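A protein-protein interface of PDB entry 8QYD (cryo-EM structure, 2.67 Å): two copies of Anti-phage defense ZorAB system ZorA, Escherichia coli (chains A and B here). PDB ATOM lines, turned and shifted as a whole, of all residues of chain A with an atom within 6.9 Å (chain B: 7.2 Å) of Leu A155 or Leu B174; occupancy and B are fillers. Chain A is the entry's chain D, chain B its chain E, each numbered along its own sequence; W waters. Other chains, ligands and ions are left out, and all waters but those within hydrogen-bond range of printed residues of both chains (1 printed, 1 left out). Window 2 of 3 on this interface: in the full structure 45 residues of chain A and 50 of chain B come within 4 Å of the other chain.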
ATOM      1  N   LEU A   8       0.463  17.025 -28.740  1.00  0.00           N
ATOM      2  CA  LEU A   8      -0.738  17.827 -28.536  1.00  0.00           C
ATOM      3  C   LEU A   8      -0.443  19.317 -28.644  1.00  0.00           C
ATOM      4  O   LEU A   8      -1.223  20.063 -29.245  1.00  0.00           O
ATOM      5  CB  LEU A   8      -1.368  17.511 -27.182  1.00  0.00           C
ATOM      6  CG  LEU A   8      -2.870  17.791 -27.139  1.00  0.00           C
ATOM      7  CD1 LEU A   8      -3.626  16.718 -27.901  1.00  0.00           C
ATOM      8  CD2 LEU A   8      -3.372  17.904 -25.711  1.00  0.00           C
ATOM      9  N   GLY A 150     -10.102  21.436 -37.401  1.00  0.00           N
ATOM     10  CA  GLY A 150     -10.264  22.879 -37.433  1.00  0.00           C
ATOM     11  C   GLY A 150     -11.232  23.391 -36.384  1.00  0.00           C
ATOM     12  O   GLY A 150     -11.002  24.438 -35.773  1.00  0.00           O
ATOM     13  N   LEU A 151     -12.326  22.663 -36.157  1.00  0.00           N
ATOM     14  CA  LEU A 151     -13.291  23.079 -35.146  1.00  0.00           C
ATOM     15  C   LEU A 151     -12.715  22.933 -33.743  1.00  0.00           C
ATOM     16  O   LEU A 151     -12.999  23.753 -32.864  1.00  0.00           O
ATOM     17  CB  LEU A 151     -14.581  22.275 -35.301  1.00  0.00           C
ATOM     18  CG  LEU A 151     -15.474  22.705 -36.467  1.00  0.00           C
ATOM     19  CD1 LEU A 151     -16.707  21.832 -36.568  1.00  0.00           C
ATOM     20  CD2 LEU A 151     -15.869  24.161 -36.335  1.00  0.00           C
ATOM     21  N   MET A 152     -11.895  21.904 -33.514  1.00  0.00           N
ATOM     22  CA  MET A 152     -11.180  21.795 -32.248  1.00  0.00           C
ATOM     23  C   MET A 152     -10.229  22.965 -32.043  1.00  0.00           C
ATOM     24  O   MET A 152     -10.146  23.514 -30.940  1.00  0.00           O
ATOM     25  CB  MET A 152     -10.424  20.470 -32.180  1.00  0.00           C
ATOM     26  CG  MET A 152     -11.292  19.273 -31.862  1.00  0.00           C
ATOM     27  SD  MET A 152     -11.662  19.181 -30.102  1.00  0.00           S
ATOM     28  CE  MET A 152     -13.244  20.000 -30.028  1.00  0.00           C
ATOM     29  N   ILE A 153      -9.498  23.357 -33.086  1.00  0.00           N
ATOM     30  CA  ILE A 153      -8.605  24.509 -32.968  1.00  0.00           C
ATOM     31  C   ILE A 153      -9.406  25.762 -32.635  1.00  0.00           C
ATOM     32  O   ILE A 153      -9.038  26.547 -31.747  1.00  0.00           O
ATOM     33  CB  ILE A 153      -7.791  24.690 -34.261  1.00  0.00           C
ATOM     34  CG1 ILE A 153      -6.794  23.548 -34.436  1.00  0.00           C
ATOM     35  CG2 ILE A 153      -7.063  26.022 -34.251  1.00  0.00           C
ATOM     36  CD1 ILE A 153      -6.073  23.583 -35.761  1.00  0.00           C
ATOM     37  N   GLY A 154     -10.525  25.954 -33.333  1.00  0.00           N
ATOM     38  CA  GLY A 154     -11.350  27.125 -33.092  1.00  0.00           C
ATOM     39  C   GLY A 154     -11.909  27.173 -31.685  1.00  0.00           C
ATOM     40  O   GLY A 154     -11.943  28.235 -31.060  1.00  0.00           O
ATOM     41  N   LEU A 155     -12.359  26.030 -31.166  1.00  0.00           N
ATOM     42  CA  LEU A 155     -12.898  26.009 -29.810  1.00  0.00           C
ATOM     43  C   LEU A 155     -11.798  26.172 -28.770  1.00  0.00           C
ATOM     44  O   LEU A 155     -12.020  26.789 -27.723  1.00  0.00           O
ATOM     45  CB  LEU A 155     -13.688  24.725 -29.572  1.00  0.00           C
ATOM     46  CG  LEU A 155     -14.968  24.596 -30.396  1.00  0.00           C
ATOM     47  CD1 LEU A 155     -15.604  23.237 -30.199  1.00  0.00           C
ATOM     48  CD2 LEU A 155     -15.938  25.696 -30.023  1.00  0.00           C
ATOM     49  N   ASN A 156     -10.608  25.628 -29.033  1.00  0.00           N
ATOM     50  CA  ASN A 156      -9.491  25.829 -28.118  1.00  0.00           C
ATOM     51  C   ASN A 156      -9.119  27.298 -28.019  1.00  0.00           C
ATOM     52  O   ASN A 156      -8.834  27.801 -26.926  1.00  0.00           O
ATOM     53  CB  ASN A 156      -8.286  25.002 -28.561  1.00  0.00           C
ATOM     54  CG  ASN A 156      -8.489  23.518 -28.353  1.00  0.00           C
ATOM     55  OD1 ASN A 156      -9.016  23.093 -27.328  1.00  0.00           O
ATOM     56  ND2 ASN A 156      -8.068  22.720 -29.326  1.00  0.00           N
ATOM     57  N   HIS A 157      -9.110  28.007 -29.147  1.00  0.00           N
ATOM     58  CA  HIS A 157      -8.774  29.424 -29.095  1.00  0.00           C
ATOM     59  C   HIS A 157      -9.893  30.273 -28.509  1.00  0.00           C
ATOM     60  O   HIS A 157      -9.635  31.399 -28.076  1.00  0.00           O
ATOM     61  CB  HIS A 157      -8.408  29.929 -30.489  1.00  0.00           C
ATOM     62  CG  HIS A 157      -7.097  29.411 -30.989  1.00  0.00           C
ATOM     63  ND1 HIS A 157      -6.024  29.178 -30.156  1.00  0.00           N
ATOM     64  CD2 HIS A 157      -6.683  29.083 -32.236  1.00  0.00           C
ATOM     65  CE1 HIS A 157      -5.007  28.726 -30.869  1.00  0.00           C
ATOM     66  NE2 HIS A 157      -5.381  28.660 -32.133  1.00  0.00           N
ATOM     67  N   PHE A 158     -11.121  29.762 -28.471  1.00  0.00           N
ATOM     68  CA  PHE A 158     -12.271  30.544 -28.027  1.00  0.00           C
ATOM     69  C   PHE A 158     -12.387  30.459 -26.511  1.00  0.00           C
ATOM     70  O   PHE A 158     -12.725  29.405 -25.964  1.00  0.00           O
ATOM     71  CB  PHE A 158     -13.543  30.045 -28.704  1.00  0.00           C
ATOM     72  CG  PHE A 158     -14.793  30.731 -28.235  1.00  0.00           C
ATOM     73  CD1 PHE A 158     -15.144  31.970 -28.729  1.00  0.00           C
ATOM     74  CD2 PHE A 158     -15.620  30.130 -27.308  1.00  0.00           C
ATOM     75  CE1 PHE A 158     -16.291  32.600 -28.302  1.00  0.00           C
ATOM     76  CE2 PHE A 158     -16.767  30.753 -26.880  1.00  0.00           C
ATOM     77  CZ  PHE A 158     -17.102  31.992 -27.377  1.00  0.00           C
ATOM     78  N   ASP A 159     -12.115  31.568 -25.831  1.00  0.00           N
ATOM     79  CA  ASP A 159     -12.196  31.625 -24.378  1.00  0.00           C
ATOM     80  C   ASP A 159     -12.334  33.072 -23.921  1.00  0.00           C
ATOM     81  O   ASP A 159     -11.330  33.714 -23.594  1.00  0.00           O
ATOM     82  CB  ASP A 159     -10.959  30.987 -23.746  1.00  0.00           C
ATOM     83  CG  ASP A 159     -11.160  30.646 -22.281  1.00  0.00           C
ATOM     84  OD1 ASP A 159     -10.377  29.829 -21.753  1.00  0.00           O
ATOM     85  OD2 ASP A 159     -12.102  31.181 -21.662  1.00  0.00           O
ATOM     86  N   LEU A 173     -13.412  32.929 -33.568  1.00  0.00           N
ATOM     87  CA  LEU A 173     -14.070  31.635 -33.683  1.00  0.00           C
ATOM     88  C   LEU A 173     -14.773  31.494 -35.022  1.00  0.00           C
ATOM     89  O   LEU A 173     -14.734  30.424 -35.639  1.00  0.00           O
ATOM     90  CB  LEU A 173     -15.065  31.456 -32.541  1.00  0.00           C
ATOM     91  CG  LEU A 173     -15.949  30.217 -32.620  1.00  0.00           C
ATOM     92  CD1 LEU A 173     -15.132  28.950 -32.467  1.00  0.00           C
ATOM     93  CD2 LEU A 173     -17.015  30.303 -31.568  1.00  0.00           C
ATOM     94  N   ASP A 176     -12.188  30.721 -37.688  1.00  0.00           N
ATOM     95  CA  ASP A 176     -11.741  29.331 -37.640  1.00  0.00           C
ATOM     96  C   ASP A 176     -12.812  28.378 -38.169  1.00  0.00           C
ATOM     97  O   ASP A 176     -12.505  27.422 -38.901  1.00  0.00           O
ATOM     98  CB  ASP A 176     -11.347  28.966 -36.212  1.00  0.00           C
ATOM     99  CG  ASP A 176     -10.177  29.784 -35.708  1.00  0.00           C
ATOM    100  OD1 ASP A 176      -9.428  30.323 -36.548  1.00  0.00           O
ATOM    101  OD2 ASP A 176     -10.003  29.889 -34.478  1.00  0.00           O
ATOM    102  N   VAL A 177     -14.073  28.624 -37.809  1.00  0.00           N
ATOM    103  CA  VAL A 177     -15.170  27.811 -38.323  1.00  0.00           C
ATOM    104  C   VAL A 177     -15.270  27.950 -39.835  1.00  0.00           C
ATOM    105  O   VAL A 177     -15.569  26.982 -40.543  1.00  0.00           O
ATOM    106  CB  VAL A 177     -16.489  28.191 -37.628  1.00  0.00           C
ATOM    107  CG1 VAL A 177     -17.654  27.515 -38.312  1.00  0.00           C
ATOM    108  CG2 VAL A 177     -16.442  27.800 -36.169  1.00  0.00           C
ATOM    109  N   GLY B 154     -14.140  14.166 -20.699  1.00  0.00           N
ATOM    110  CA  GLY B 154     -14.259  15.608 -20.552  1.00  0.00           C
ATOM    111  C   GLY B 154     -15.568  16.038 -19.916  1.00  0.00           C
ATOM    112  O   GLY B 154     -15.605  16.997 -19.142  1.00  0.00           O
ATOM    113  N   SER B 167     -14.635  27.954 -17.355  1.00  0.00           N
ATOM    114  CA  SER B 167     -13.578  28.101 -18.351  1.00  0.00           C
ATOM    115  C   SER B 167     -12.572  26.960 -18.267  1.00  0.00           C
ATOM    116  O   SER B 167     -12.166  26.394 -19.290  1.00  0.00           O
ATOM    117  CB  SER B 167     -12.881  29.449 -18.175  1.00  0.00           C
ATOM    118  OG  SER B 167     -13.830  30.497 -18.095  1.00  0.00           O
ATOM    119  N   SER B 168     -12.156  26.605 -17.047  1.00  0.00           N
ATOM    120  CA  SER B 168     -11.207  25.508 -16.891  1.00  0.00           C
ATOM    121  C   SER B 168     -11.812  24.188 -17.352  1.00  0.00           C
ATOM    122  O   SER B 168     -11.129  23.370 -17.977  1.00  0.00           O
ATOM    123  CB  SER B 168     -10.746  25.409 -15.440  1.00  0.00           C
ATOM    124  OG  SER B 168     -11.817  25.053 -14.589  1.00  0.00           O
ATOM    125  N   SER B 169     -13.092  23.961 -17.049  1.00  0.00           N
ATOM    126  CA  SER B 169     -13.751  22.734 -17.475  1.00  0.00           C
ATOM    127  C   SER B 169     -13.863  22.666 -18.989  1.00  0.00           C
ATOM    128  O   SER B 169     -13.693  21.597 -19.581  1.00  0.00           O
ATOM    129  CB  SER B 169     -15.128  22.636 -16.827  1.00  0.00           C
ATOM    130  OG  SER B 169     -15.020  22.629 -15.416  1.00  0.00           O
ATOM    131  N   VAL B 170     -14.158  23.795 -19.634  1.00  0.00           N
ATOM    132  CA  VAL B 170     -14.211  23.822 -21.094  1.00  0.00           C
ATOM    133  C   VAL B 170     -12.843  23.497 -21.676  1.00  0.00           C
ATOM    134  O   VAL B 170     -12.724  22.715 -22.626  1.00  0.00           O
ATOM    135  CB  VAL B 170     -14.731  25.182 -21.591  1.00  0.00           C
ATOM    136  CG1 VAL B 170     -14.447  25.348 -23.071  1.00  0.00           C
ATOM    137  CG2 VAL B 170     -16.218  25.302 -21.326  1.00  0.00           C
ATOM    138  N   ASN B 171     -11.789  24.088 -21.110  1.00  0.00           N
ATOM    139  CA  ASN B 171     -10.443  23.797 -21.597  1.00  0.00           C
ATOM    140  C   ASN B 171     -10.102  22.321 -21.434  1.00  0.00           C
ATOM    141  O   ASN B 171      -9.554  21.699 -22.350  1.00  0.00           O
ATOM    142  CB  ASN B 171      -9.418  24.663 -20.869  1.00  0.00           C
ATOM    143  CG  ASN B 171      -9.513  26.119 -21.252  1.00  0.00           C
ATOM    144  OD1 ASN B 171      -9.688  26.452 -22.422  1.00  0.00           O
ATOM    145  ND2 ASN B 171      -9.392  26.999 -20.268  1.00  0.00           N
ATOM    146  N   ASN B 172     -10.427  21.742 -20.276  1.00  0.00           N
ATOM    147  CA  ASN B 172     -10.122  20.335 -20.036  1.00  0.00           C
ATOM    148  C   ASN B 172     -10.913  19.428 -20.970  1.00  0.00           C
ATOM    149  O   ASN B 172     -10.379  18.441 -21.490  1.00  0.00           O
ATOM    150  CB  ASN B 172     -10.406  19.980 -18.580  1.00  0.00           C
ATOM    151  CG  ASN B 172      -9.543  20.758 -17.613  1.00  0.00           C
ATOM    152  OD1 ASN B 172      -8.441  21.182 -17.953  1.00  0.00           O
ATOM    153  ND2 ASN B 172     -10.037  20.946 -16.398  1.00  0.00           N
ATOM    154  N   LEU B 173     -12.191  19.744 -21.188  1.00  0.00           N
ATOM    155  CA  LEU B 173     -13.012  18.955 -22.097  1.00  0.00           C
ATOM    156  C   LEU B 173     -12.469  19.007 -23.516  1.00  0.00           C
ATOM    157  O   LEU B 173     -12.380  17.976 -24.194  1.00  0.00           O
ATOM    158  CB  LEU B 173     -14.454  19.457 -22.049  1.00  0.00           C
ATOM    159  CG  LEU B 173     -15.409  19.075 -23.175  1.00  0.00           C
ATOM    160  CD1 LEU B 173     -15.627  17.579 -23.230  1.00  0.00           C
ATOM    161  CD2 LEU B 173     -16.726  19.794 -22.993  1.00  0.00           C
ATOM    162  N   LEU B 174     -12.094  20.200 -23.981  1.00  0.00           N
ATOM    163  CA  LEU B 174     -11.538  20.321 -25.322  1.00  0.00           C
ATOM    164  C   LEU B 174     -10.211  19.587 -25.440  1.00  0.00           C
ATOM    165  O   LEU B 174      -9.927  18.975 -26.472  1.00  0.00           O
ATOM    166  CB  LEU B 174     -11.381  21.793 -25.694  1.00  0.00           C
ATOM    167  CG  LEU B 174     -12.676  22.594 -25.780  1.00  0.00           C
ATOM    168  CD1 LEU B 174     -12.369  24.058 -25.985  1.00  0.00           C
ATOM    169  CD2 LEU B 174     -13.552  22.068 -26.897  1.00  0.00           C
ATOM    170  N   ARG B 175      -9.386  19.629 -24.392  1.00  0.00           N
ATOM    171  CA  ARG B 175      -8.119  18.903 -24.419  1.00  0.00           C
ATOM    172  C   ARG B 175      -8.333  17.395 -24.498  1.00  0.00           C
ATOM    173  O   ARG B 175      -7.652  16.703 -25.270  1.00  0.00           O
ATOM    174  CB  ARG B 175      -7.295  19.260 -23.185  1.00  0.00           C
ATOM    175  CG  ARG B 175      -5.909  18.660 -23.173  1.00  0.00           C
ATOM    176  CD  ARG B 175      -5.139  19.115 -21.954  1.00  0.00           C
ATOM    177  NE  ARG B 175      -5.749  18.624 -20.726  1.00  0.00           N
ATOM    178  CZ  ARG B 175      -6.317  19.398 -19.813  1.00  0.00           C
ATOM    179  NH1 ARG B 175      -6.361  20.713 -19.952  1.00  0.00           N
ATOM    180  NH2 ARG B 175      -6.854  18.839 -18.732  1.00  0.00           N
ATOM    181  N   ASP B 176      -9.263  16.865 -23.698  1.00  0.00           N
ATOM    182  CA  ASP B 176      -9.540  15.433 -23.735  1.00  0.00           C
ATOM    183  C   ASP B 176     -10.089  15.013 -25.091  1.00  0.00           C
ATOM    184  O   ASP B 176      -9.673  13.989 -25.653  1.00  0.00           O
ATOM    185  CB  ASP B 176     -10.518  15.058 -22.625  1.00  0.00           C
ATOM    186  CG  ASP B 176     -10.018  15.450 -21.253  1.00  0.00           C
ATOM    187  OD1 ASP B 176      -8.868  15.921 -21.152  1.00  0.00           O
ATOM    188  OD2 ASP B 176     -10.775  15.293 -20.274  1.00  0.00           O
ATOM    189  N   VAL B 177     -11.018  15.799 -25.642  1.00  0.00           N
ATOM    190  CA  VAL B 177     -11.546  15.481 -26.962  1.00  0.00           C
ATOM    191  C   VAL B 177     -10.457  15.598 -28.019  1.00  0.00           C
ATOM    192  O   VAL B 177     -10.473  14.868 -29.011  1.00  0.00           O
ATOM    193  CB  VAL B 177     -12.757  16.372 -27.294  1.00  0.00           C
ATOM    194  CG1 VAL B 177     -13.244  16.098 -28.702  1.00  0.00           C
ATOM    195  CG2 VAL B 177     -13.877  16.134 -26.301  1.00  0.00           C
ATOM    196  N   LEU B 178      -9.492  16.498 -27.828  1.00  0.00           N
ATOM    197  CA  LEU B 178      -8.414  16.641 -28.800  1.00  0.00           C
ATOM    198  C   LEU B 178      -7.495  15.425 -28.791  1.00  0.00           C
ATOM    199  O   LEU B 178      -7.093  14.938 -29.853  1.00  0.00           O
ATOM    200  CB  LEU B 178      -7.632  17.920 -28.514  1.00  0.00           C
ATOM    201  CG  LEU B 178      -6.598  18.371 -29.539  1.00  0.00           C
ATOM    202  CD1 LEU B 178      -7.285  18.802 -30.821  1.00  0.00           C
ATOM    203  CD2 LEU B 178      -5.778  19.503 -28.971  1.00  0.00           C
ATOM    204  N   TYR B 179      -7.153  14.922 -27.602  1.00  0.00           N
ATOM    205  CA  TYR B 179      -6.449  13.642 -27.506  1.00  0.00           C
ATOM    206  C   TYR B 179      -7.216  12.537 -28.227  1.00  0.00           C
ATOM    207  O   TYR B 179      -6.666  11.799 -29.064  1.00  0.00           O
ATOM    208  CB  TYR B 179      -6.270  13.259 -26.037  1.00  0.00           C
ATOM    209  CG  TYR B 179      -5.117  13.898 -25.303  1.00  0.00           C
ATOM    210  CD1 TYR B 179      -3.834  13.876 -25.826  1.00  0.00           C
ATOM    211  CD2 TYR B 179      -5.309  14.495 -24.066  1.00  0.00           C
ATOM    212  CE1 TYR B 179      -2.778  14.444 -25.143  1.00  0.00           C
ATOM    213  CE2 TYR B 179      -4.264  15.068 -23.379  1.00  0.00           C
ATOM    214  CZ  TYR B 179      -3.000  15.039 -23.919  1.00  0.00           C
ATOM    215  OH  TYR B 179      -1.954  15.610 -23.234  1.00  0.00           O
ATOM    216  N   ALA B 180      -8.499  12.403 -27.891  1.00  0.00           N
ATOM    217  CA  ALA B 180      -9.307  11.336 -28.462  1.00  0.00           C
ATOM    218  C   ALA B 180      -9.384  11.455 -29.977  1.00  0.00           C
ATOM    219  O   ALA B 180      -9.333  10.447 -30.690  1.00  0.00           O
ATOM    220  CB  ALA B 180     -10.697  11.362 -27.838  1.00  0.00           C
HETATM  221  O   HOH W   1     -13.052  28.266 -22.004  1.00  0.00           O
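OD1 of Asp A159 is in hydrogen-bond range of ND2 of Asn B171 (3.3 Å).
The backbone carbonyl oxygen (O) of Met A152 lies within hydrogen-bond range of the side-chain amide nitrogen (ND2) of Asn A156, at 2.7 Å.
O of Ser B167 sits at hydrogen-bond distance from ND2 of Asn B171 (3.0 Å).
OD1 of Asn B172 sits at hydrogen-bond distance from NH1 of Arg B175 (2.9 Å).
Arg B175 touches Leu A8 (CG to CD2, 3.7 Å).
Leu A8 touches Leu B178.
CZ of Tyr B179 touches CD2 of Leu A8 (3.4 Å).
Met A152 touches Leu B174 (CE to CD2, 3.8 Å).
Val B177 touches Met A152 (CG1 to SD, 3.7 Å).
CD1 of Leu B178 touches CB of Met A152, at 3.8 Å.
O of Leu A155 touches CD1 of Leu B174, 3.3 Å away.
CB of Leu B174 touches OD1 of Asn A156, at 3.2 Å.
Asn A156 touches Leu B178 (ND2 to CD2, 3.96 Å).
CB of Ser B167 touches OD2 of Asp A159, at 3.97 Å.
Of the printed residues of chain B, Leu A155 touches Leu B174.
No residue of chain B comes within 4 Å of Gly A154.
Of the printed residues of chain A, Ser B167 touches Asp A159.
Printed residues of chain A within 4 Å of Asn B171: Asp A159 (3.3 Å).
Printed residues of chain A within 4 Å of Val B177: Met A152 (3.7 Å).
Of the printed residues of chain B, Leu A8 touches Arg B175, Leu B178 and Tyr B179.
Asp B176 touches none of the printed residues of chain A.
Leu B173 touches none of the printed residues of chain A.
The nearest residue of chain A that does not touch Leu B174 is Phe A158 (5.4 Å).
The nearest printed residue of chain B that does not touch Asp A159 is Ser B168 (6.0 Å).
Of the 15 printed residues of chain B, 7 touch a printed residue of chain A.
Hydrophobic or aromatic side chains of chain B that line the printed part of chain A: Leu B174, Val B177, Leu B178 and Tyr B179.
Among the printed residues, 11 pairs touch across the chains.
4 positions are printed for both chains.
Of the 11 pairs that touch across the chains among the printed residues, none has its exchanged pair printed and touching as well.
Water W1 lies within hydrogen-bond range of the side-chain carboxylate of Asp A159 (3.1 Å) and the backbone carbonyl oxygen of Ser B167 (3.4 Å).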
